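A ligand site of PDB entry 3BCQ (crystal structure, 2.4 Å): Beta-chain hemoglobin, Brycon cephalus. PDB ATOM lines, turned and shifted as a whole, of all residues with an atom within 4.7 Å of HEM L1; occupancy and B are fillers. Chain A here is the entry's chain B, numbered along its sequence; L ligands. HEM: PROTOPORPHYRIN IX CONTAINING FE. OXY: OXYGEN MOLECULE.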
ATOM      1  N   LEU A  31      15.983  16.649  29.838  1.00  0.00           N
ATOM      2  CA  LEU A  31      15.606  15.274  30.110  1.00  0.00           C
ATOM      3  C   LEU A  31      15.418  15.036  31.593  1.00  0.00           C
ATOM      4  O   LEU A  31      14.493  14.436  32.003  1.00  0.00           O
ATOM      5  CB  LEU A  31      16.692  14.336  29.624  1.00  0.00           C
ATOM      6  CG  LEU A  31      16.375  12.874  29.788  1.00  0.00           C
ATOM      7  CD1 LEU A  31      15.489  12.464  28.604  1.00  0.00           C
ATOM      8  CD2 LEU A  31      17.686  12.065  29.843  1.00  0.00           C
ATOM      9  N   THR A  38      14.330   9.423  34.967  1.00  0.00           N
ATOM     10  CA  THR A  38      15.581   9.280  34.221  1.00  0.00           C
ATOM     11  C   THR A  38      16.733   9.689  35.212  1.00  0.00           C
ATOM     12  O   THR A  38      17.831   9.303  35.048  1.00  0.00           O
ATOM     13  CB  THR A  38      15.362  10.275  33.081  1.00  0.00           C
ATOM     14  OG1 THR A  38      15.420   9.665  31.781  1.00  0.00           O
ATOM     15  CG2 THR A  38      16.056  11.469  33.257  1.00  0.00           C
ATOM     16  N   HIS A  41      18.926   6.902  36.882  1.00  0.00           N
ATOM     17  CA  HIS A  41      20.170   6.445  36.247  1.00  0.00           C
ATOM     18  C   HIS A  41      21.378   7.264  36.589  1.00  0.00           C
ATOM     19  O   HIS A  41      22.463   6.828  36.440  1.00  0.00           O
ATOM     20  CB  HIS A  41      19.994   6.421  34.733  1.00  0.00           C
ATOM     21  CG  HIS A  41      18.957   5.449  34.289  1.00  0.00           C
ATOM     22  ND1 HIS A  41      19.148   4.090  34.373  1.00  0.00           N
ATOM     23  CD2 HIS A  41      17.705   5.623  33.807  1.00  0.00           C
ATOM     24  CE1 HIS A  41      18.058   3.460  33.978  1.00  0.00           C
ATOM     25  NE2 HIS A  41      17.172   4.367  33.602  1.00  0.00           N
ATOM     26  N   PHE A  42      21.165   8.494  37.012  1.00  0.00           N
ATOM     27  CA  PHE A  42      22.245   9.402  37.313  1.00  0.00           C
ATOM     28  C   PHE A  42      22.227   9.722  38.807  1.00  0.00           C
ATOM     29  O   PHE A  42      22.500  10.841  39.147  1.00  0.00           O
ATOM     30  CB  PHE A  42      21.995  10.748  36.563  1.00  0.00           C
ATOM     31  CG  PHE A  42      21.923  10.584  35.102  1.00  0.00           C
ATOM     32  CD1 PHE A  42      23.070  10.560  34.357  1.00  0.00           C
ATOM     33  CD2 PHE A  42      20.717  10.375  34.479  1.00  0.00           C
ATOM     34  CE1 PHE A  42      23.030  10.347  32.983  1.00  0.00           C
ATOM     35  CE2 PHE A  42      20.641  10.183  33.101  1.00  0.00           C
ATOM     36  CZ  PHE A  42      21.797  10.177  32.347  1.00  0.00           C
ATOM     37  N   PHE A  45      25.215  11.537  40.555  1.00  0.00           N
ATOM     38  CA  PHE A  45      25.458  12.941  40.126  1.00  0.00           C
ATOM     39  C   PHE A  45      25.214  14.089  41.124  1.00  0.00           C
ATOM     40  O   PHE A  45      25.617  15.206  40.836  1.00  0.00           O
ATOM     41  CB  PHE A  45      24.668  13.242  38.813  1.00  0.00           C
ATOM     42  CG  PHE A  45      25.277  12.624  37.568  1.00  0.00           C
ATOM     43  CD1 PHE A  45      25.887  11.381  37.615  1.00  0.00           C
ATOM     44  CD2 PHE A  45      25.223  13.298  36.349  1.00  0.00           C
ATOM     45  CE1 PHE A  45      26.440  10.812  36.493  1.00  0.00           C
ATOM     46  CE2 PHE A  45      25.785  12.729  35.192  1.00  0.00           C
ATOM     47  CZ  PHE A  45      26.388  11.489  35.260  1.00  0.00           C
ATOM     48  N   LYS A  59      28.352  17.803  37.012  1.00  0.00           N
ATOM     49  CA  LYS A  59      28.422  16.468  36.468  1.00  0.00           C
ATOM     50  C   LYS A  59      27.379  16.297  35.372  1.00  0.00           C
ATOM     51  O   LYS A  59      27.665  15.669  34.341  1.00  0.00           O
ATOM     52  CB  LYS A  59      28.332  15.413  37.578  1.00  0.00           C
ATOM     53  CG  LYS A  59      29.293  14.198  37.333  1.00  0.00           C
ATOM     54  CD  LYS A  59      29.257  13.218  38.492  1.00  0.00           C
ATOM     55  CE  LYS A  59      29.485  11.751  37.995  1.00  0.00           C
ATOM     56  NZ  LYS A  59      30.788  11.435  37.366  1.00  0.00           N
ATOM     57  N   HIS A  63      28.454  15.776  31.674  1.00  0.00           N
ATOM     58  CA  HIS A  63      27.959  14.607  31.022  1.00  0.00           C
ATOM     59  C   HIS A  63      27.142  14.933  29.746  1.00  0.00           C
ATOM     60  O   HIS A  63      27.128  14.163  28.810  1.00  0.00           O
ATOM     61  CB  HIS A  63      27.176  13.754  31.996  1.00  0.00           C
ATOM     62  CG  HIS A  63      26.711  12.488  31.361  1.00  0.00           C
ATOM     63  ND1 HIS A  63      27.566  11.419  31.136  1.00  0.00           N
ATOM     64  CD2 HIS A  63      25.530  12.152  30.799  1.00  0.00           C
ATOM     65  CE1 HIS A  63      26.908  10.470  30.494  1.00  0.00           C
ATOM     66  NE2 HIS A  63      25.672  10.894  30.273  1.00  0.00           N
ATOM     67  N   VAL A  66      29.583  15.063  27.172  1.00  0.00           N
ATOM     68  CA  VAL A  66      29.997  13.691  26.846  1.00  0.00           C
ATOM     69  C   VAL A  66      28.970  13.041  25.922  1.00  0.00           C
ATOM     70  O   VAL A  66      29.320  12.332  24.963  1.00  0.00           O
ATOM     71  CB  VAL A  66      30.254  12.813  28.129  1.00  0.00           C
ATOM     72  CG1 VAL A  66      30.477  11.392  27.765  1.00  0.00           C
ATOM     73  CG2 VAL A  66      31.471  13.321  28.911  1.00  0.00           C
ATOM     74  N   VAL A  67      27.691  13.247  26.209  1.00  0.00           N
ATOM     75  CA  VAL A  67      26.630  12.864  25.214  1.00  0.00           C
ATOM     76  C   VAL A  67      26.854  13.464  23.820  1.00  0.00           C
ATOM     77  O   VAL A  67      26.771  12.753  22.852  1.00  0.00           O
ATOM     78  CB  VAL A  67      25.209  13.184  25.684  1.00  0.00           C
ATOM     79  CG1 VAL A  67      24.172  12.938  24.553  1.00  0.00           C
ATOM     80  CG2 VAL A  67      24.884  12.434  26.996  1.00  0.00           C
ATOM     81  N   GLY A  70      29.348  11.423  22.133  1.00  0.00           N
ATOM     82  CA  GLY A  70      28.765  10.234  21.509  1.00  0.00           C
ATOM     83  C   GLY A  70      28.159  10.524  20.117  1.00  0.00           C
ATOM     84  O   GLY A  70      28.333   9.715  19.150  1.00  0.00           O
ATOM     85  N   LEU A  71      27.496  11.690  19.984  1.00  0.00           N
ATOM     86  CA  LEU A  71      26.932  12.092  18.727  1.00  0.00           C
ATOM     87  C   LEU A  71      27.993  12.420  17.673  1.00  0.00           C
ATOM     88  O   LEU A  71      27.881  11.969  16.537  1.00  0.00           O
ATOM     89  CB  LEU A  71      25.983  13.278  18.881  1.00  0.00           C
ATOM     90  CG  LEU A  71      24.758  13.066  19.731  1.00  0.00           C
ATOM     91  CD1 LEU A  71      23.751  14.067  19.287  1.00  0.00           C
ATOM     92  CD2 LEU A  71      24.220  11.660  19.524  1.00  0.00           C
ATOM     93  N   TYR A  85      29.142   2.173  17.940  1.00  0.00           N
ATOM     94  CA  TYR A  85      28.389   2.290  19.184  1.00  0.00           C
ATOM     95  C   TYR A  85      28.391   0.982  19.953  1.00  0.00           C
ATOM     96  O   TYR A  85      27.836   0.878  21.063  1.00  0.00           O
ATOM     97  CB  TYR A  85      26.965   2.736  18.852  1.00  0.00           C
ATOM     98  CG  TYR A  85      26.823   4.198  18.925  1.00  0.00           C
ATOM     99  CD1 TYR A  85      27.752   5.033  18.327  1.00  0.00           C
ATOM    100  CD2 TYR A  85      25.744   4.788  19.578  1.00  0.00           C
ATOM    101  CE1 TYR A  85      27.682   6.366  18.405  1.00  0.00           C
ATOM    102  CE2 TYR A  85      25.651   6.149  19.679  1.00  0.00           C
ATOM    103  CZ  TYR A  85      26.626   6.931  19.074  1.00  0.00           C
ATOM    104  OH  TYR A  85      26.539   8.311  19.098  1.00  0.00           O
ATOM    105  N   LEU A  88      29.050   1.176  23.561  1.00  0.00           N
ATOM    106  CA  LEU A  88      27.978   2.016  24.082  1.00  0.00           C
ATOM    107  C   LEU A  88      26.652   1.269  24.261  1.00  0.00           C
ATOM    108  O   LEU A  88      26.071   1.310  25.336  1.00  0.00           O
ATOM    109  CB  LEU A  88      27.813   3.214  23.188  1.00  0.00           C
ATOM    110  CG  LEU A  88      28.850   4.307  23.405  1.00  0.00           C
ATOM    111  CD1 LEU A  88      28.403   5.601  22.681  1.00  0.00           C
ATOM    112  CD2 LEU A  88      29.029   4.477  24.935  1.00  0.00           C
ATOM    113  N   MET A  91      27.062  -1.096  27.205  1.00  0.00           N
ATOM    114  CA  MET A  91      27.014  -0.335  28.456  1.00  0.00           C
ATOM    115  C   MET A  91      25.590   0.186  28.797  1.00  0.00           C
ATOM    116  O   MET A  91      25.209   0.131  29.964  1.00  0.00           O
ATOM    117  CB  MET A  91      28.045   0.809  28.454  1.00  0.00           C
ATOM    118  CG  MET A  91      28.209   1.559  29.833  1.00  0.00           C
ATOM    119  SD  MET A  91      28.672   3.282  29.525  1.00  0.00           S
ATOM    120  CE  MET A  91      28.213   4.070  31.082  1.00  0.00           C
ATOM    121  N   HIS A  92      24.827   0.638  27.794  1.00  0.00           N
ATOM    122  CA  HIS A  92      23.443   1.063  27.999  1.00  0.00           C
ATOM    123  C   HIS A  92      22.386  -0.089  28.060  1.00  0.00           C
ATOM    124  O   HIS A  92      21.434   0.024  28.830  1.00  0.00           O
ATOM    125  CB  HIS A  92      23.012   2.136  26.982  1.00  0.00           C
ATOM    126  CG  HIS A  92      23.664   3.471  27.185  1.00  0.00           C
ATOM    127  ND1 HIS A  92      24.797   3.863  26.507  1.00  0.00           N
ATOM    128  CD2 HIS A  92      23.323   4.519  27.964  1.00  0.00           C
ATOM    129  CE1 HIS A  92      25.145   5.073  26.882  1.00  0.00           C
ATOM    130  NE2 HIS A  92      24.267   5.495  27.768  1.00  0.00           N
ATOM    131  N   LEU A  96      23.763  -0.740  32.211  1.00  0.00           N
ATOM    132  CA  LEU A  96      22.853   0.211  32.857  1.00  0.00           C
ATOM    133  C   LEU A  96      21.338  -0.220  32.822  1.00  0.00           C
ATOM    134  O   LEU A  96      20.535   0.234  33.679  1.00  0.00           O
ATOM    135  CB  LEU A  96      23.048   1.649  32.343  1.00  0.00           C
ATOM    136  CG  LEU A  96      24.456   2.315  32.440  1.00  0.00           C
ATOM    137  CD1 LEU A  96      24.560   3.459  31.469  1.00  0.00           C
ATOM    138  CD2 LEU A  96      24.968   2.745  33.846  1.00  0.00           C
ATOM    139  N   VAL A  98      19.106   0.656  30.586  1.00  0.00           N
ATOM    140  CA  VAL A  98      18.368   1.851  30.309  1.00  0.00           C
ATOM    141  C   VAL A  98      17.265   1.349  29.339  1.00  0.00           C
ATOM    142  O   VAL A  98      17.553   0.810  28.260  1.00  0.00           O
ATOM    143  CB  VAL A  98      19.277   2.982  29.678  1.00  0.00           C
ATOM    144  CG1 VAL A  98      18.374   4.129  29.191  1.00  0.00           C
ATOM    145  CG2 VAL A  98      20.443   3.497  30.679  1.00  0.00           C
ATOM    146  N   ASN A 102      13.995   5.660  26.585  1.00  0.00           N
ATOM    147  CA  ASN A 102      14.731   6.770  27.072  1.00  0.00           C
ATOM    148  C   ASN A 102      15.674   7.367  26.089  1.00  0.00           C
ATOM    149  O   ASN A 102      15.887   8.565  26.114  1.00  0.00           O
ATOM    150  CB  ASN A 102      15.414   6.515  28.421  1.00  0.00           C
ATOM    151  CG  ASN A 102      14.405   6.169  29.499  1.00  0.00           C
ATOM    152  OD1 ASN A 102      13.468   6.961  29.841  1.00  0.00           O
ATOM    153  ND2 ASN A 102      14.552   4.936  30.020  1.00  0.00           N
ATOM    154  N   PHE A 103      16.266   6.573  25.219  1.00  0.00           N
ATOM    155  CA  PHE A 103      17.207   7.150  24.261  1.00  0.00           C
ATOM    156  C   PHE A 103      16.349   8.021  23.352  1.00  0.00           C
ATOM    157  O   PHE A 103      16.838   9.061  22.897  1.00  0.00           O
ATOM    158  CB  PHE A 103      17.923   6.090  23.372  1.00  0.00           C
ATOM    159  CG  PHE A 103      18.575   4.959  24.138  1.00  0.00           C
ATOM    160  CD1 PHE A 103      19.329   5.202  25.250  1.00  0.00           C
ATOM    161  CD2 PHE A 103      18.416   3.647  23.710  1.00  0.00           C
ATOM    162  CE1 PHE A 103      19.921   4.148  25.974  1.00  0.00           C
ATOM    163  CE2 PHE A 103      18.989   2.570  24.403  1.00  0.00           C
ATOM    164  CZ  PHE A 103      19.753   2.817  25.555  1.00  0.00           C
ATOM    165  N   LEU A 106      15.746  11.520  25.161  1.00  0.00           N
ATOM    166  CA  LEU A 106      16.959  12.364  25.072  1.00  0.00           C
ATOM    167  C   LEU A 106      17.189  12.936  23.725  1.00  0.00           C
ATOM    168  O   LEU A 106      17.506  14.054  23.632  1.00  0.00           O
ATOM    169  CB  LEU A 106      18.210  11.562  25.382  1.00  0.00           C
ATOM    170  CG  LEU A 106      19.369  12.293  26.100  1.00  0.00           C
ATOM    171  CD1 LEU A 106      20.645  11.686  25.753  1.00  0.00           C
ATOM    172  CD2 LEU A 106      19.463  13.835  26.132  1.00  0.00           C
ATOM    173  N   VAL A 138      21.133   6.545  15.673  1.00  0.00           N
ATOM    174  CA  VAL A 138      21.910   6.518  16.906  1.00  0.00           C
ATOM    175  C   VAL A 138      21.185   5.728  17.964  1.00  0.00           C
ATOM    176  O   VAL A 138      21.732   4.861  18.642  1.00  0.00           O
ATOM    177  CB  VAL A 138      22.164   7.965  17.412  1.00  0.00           C
ATOM    178  CG1 VAL A 138      22.571   7.991  18.897  1.00  0.00           C
ATOM    179  CG2 VAL A 138      23.221   8.577  16.547  1.00  0.00           C
ATOM    180  N   LEU A 142      22.095   2.303  19.911  1.00  0.00           N
ATOM    181  CA  LEU A 142      22.284   2.257  21.362  1.00  0.00           C
ATOM    182  C   LEU A 142      21.699   1.171  22.326  1.00  0.00           C
ATOM    183  O   LEU A 142      22.502   0.539  22.953  1.00  0.00           O
ATOM    184  CB  LEU A 142      21.965   3.625  21.967  1.00  0.00           C
ATOM    185  CG  LEU A 142      23.113   4.586  22.287  1.00  0.00           C
ATOM    186  CD1 LEU A 142      22.524   5.598  23.188  1.00  0.00           C
ATOM    187  CD2 LEU A 142      24.310   3.928  22.939  1.00  0.00           C
HETATM  188  CHA HEM L   1      27.336   7.124  29.733  1.00  0.00           C
HETATM  189  CHB HEM L   1      26.253   8.535  25.196  1.00  0.00           C
HETATM  190  CHC HEM L   1      21.564   8.214  26.348  1.00  0.00           C
HETATM  191  CHD HEM L   1      22.526   6.961  30.838  1.00  0.00           C
HETATM  192  C1A HEM L   1      27.502   7.564  28.463  1.00  0.00           C
HETATM  193  C2A HEM L   1      28.717   7.974  27.821  1.00  0.00           C
HETATM  194  C3A HEM L   1      28.398   8.361  26.580  1.00  0.00           C
HETATM  195  C4A HEM L   1      26.977   8.219  26.373  1.00  0.00           C
HETATM  196  CMA HEM L   1      29.374   8.883  25.508  1.00  0.00           C
HETATM  197  CAA HEM L   1      30.143   7.960  28.463  1.00  0.00           C
HETATM  198  CBA HEM L   1      30.700   6.564  28.179  1.00  0.00           C
HETATM  199  CGA HEM L   1      31.936   6.196  29.009  1.00  0.00           C
HETATM  200  O1A HEM L   1      32.780   5.423  28.443  1.00  0.00           O
HETATM  201  O2A HEM L   1      32.068   6.621  30.211  1.00  0.00           O
HETATM  202  C1B HEM L   1      24.896   8.565  25.105  1.00  0.00           C
HETATM  203  C2B HEM L   1      24.092   8.841  23.946  1.00  0.00           C
HETATM  204  C3B HEM L   1      22.770   8.743  24.310  1.00  0.00           C
HETATM  205  C4B HEM L   1      22.750   8.375  25.686  1.00  0.00           C
HETATM  206  CMB HEM L   1      24.664   9.181  22.563  1.00  0.00           C
HETATM  207  CAB HEM L   1      21.404   8.909  23.550  1.00  0.00           C
HETATM  208  CBB HEM L   1      21.274   9.701  22.500  1.00  0.00           C
HETATM  209  C1C HEM L   1      21.354   7.894  27.632  1.00  0.00           C
HETATM  210  C2C HEM L   1      20.090   7.791  28.258  1.00  0.00           C
HETATM  211  C3C HEM L   1      20.338   7.421  29.547  1.00  0.00           C
HETATM  212  C4C HEM L   1      21.787   7.317  29.717  1.00  0.00           C
HETATM  213  CMC HEM L   1      18.716   8.057  27.554  1.00  0.00           C
HETATM  214  CAC HEM L   1      19.248   7.113  30.614  1.00  0.00           C
HETATM  215  CBC HEM L   1      18.656   8.050  31.358  1.00  0.00           C
HETATM  216  C1D HEM L   1      23.911   6.988  31.006  1.00  0.00           C
HETATM  217  C2D HEM L   1      24.571   6.887  32.264  1.00  0.00           C
HETATM  218  C3D HEM L   1      26.043   6.960  31.958  1.00  0.00           C
HETATM  219  C4D HEM L   1      26.149   7.067  30.504  1.00  0.00           C
HETATM  220  CMD HEM L   1      23.981   6.796  33.686  1.00  0.00           C
HETATM  221  CAD HEM L   1      27.126   6.891  33.044  1.00  0.00           C
HETATM  222  CBD HEM L   1      27.388   8.170  33.865  1.00  0.00           C
HETATM  223  CGD HEM L   1      28.633   7.887  34.744  1.00  0.00           C
HETATM  224  O1D HEM L   1      28.713   6.748  35.313  1.00  0.00           O
HETATM  225  O2D HEM L   1      29.574   8.736  34.869  1.00  0.00           O
HETATM  226  NA  HEM L   1      26.497   7.726  27.554  1.00  0.00           N
HETATM  227  NB  HEM L   1      24.021   8.276  26.150  1.00  0.00           N
HETATM  228  NC  HEM L   1      22.344   7.596  28.525  1.00  0.00           N
HETATM  229  ND  HEM L   1      24.861   7.047  30.012  1.00  0.00           N
HETATM  230 FE   HEM L   1      24.383   7.652  28.107  1.00  0.00          FE
HETATM  231  O1  OXY L   2      24.538   9.186  28.586  1.00  0.00           O
HETATM  232  O2  OXY L   2      23.650  10.006  28.723  1.00  0.00           O
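An iron atom (FE) of HEM L1 is bound by a ring nitrogen (NE2) of His 92.
NZ of Lys 59 is in salt-bridge range of O2D of HEM L1 (3.9 Å).
A ring nitrogen (NE2) of His 63 lies close to an oxygen (O1) of OXY L2 (2.7 Å).
Merely in contact with HEM L1: His 41, Asn 102, Leu 142, Phe 42, Val 98, Met 91, His 63, Val 66, Leu 96, Leu 106, Thr 38, Phe 103, Phe 45 and Leu 71.
Hydrophobic or aromatic side chains that line HEM L1: His 41, Phe 42, Phe 45, His 63, Val 66, Leu 71, Met 91, His 92, Leu 96, Val 98, Phe 103, Leu 106 and Leu 142.
Within 4 Å of HEM L1: Thr 38, His 41, Phe 42, Phe 45, Lys 59, His 63, Val 66, Leu 71, Met 91, His 92, Leu 96, Val 98, Asn 102, Phe 103, Leu 106 and Leu 142.
An oxygen (O1) of OXY L2 binds an iron atom (FE) of HEM L1 (1.6 Å).
O of Met 91 sits at hydrogen-bond distance from N of Leu 96, 2.8 Å away.
The backbone carbonyl oxygen (O) of Leu 88 is in hydrogen-bond range of a ring nitrogen (ND1) of His 92.
The backbone carbonyl oxygen (O) of His 92 sits at hydrogen-bond distance from the backbone NH (N) of Val 98 (3.0 Å).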
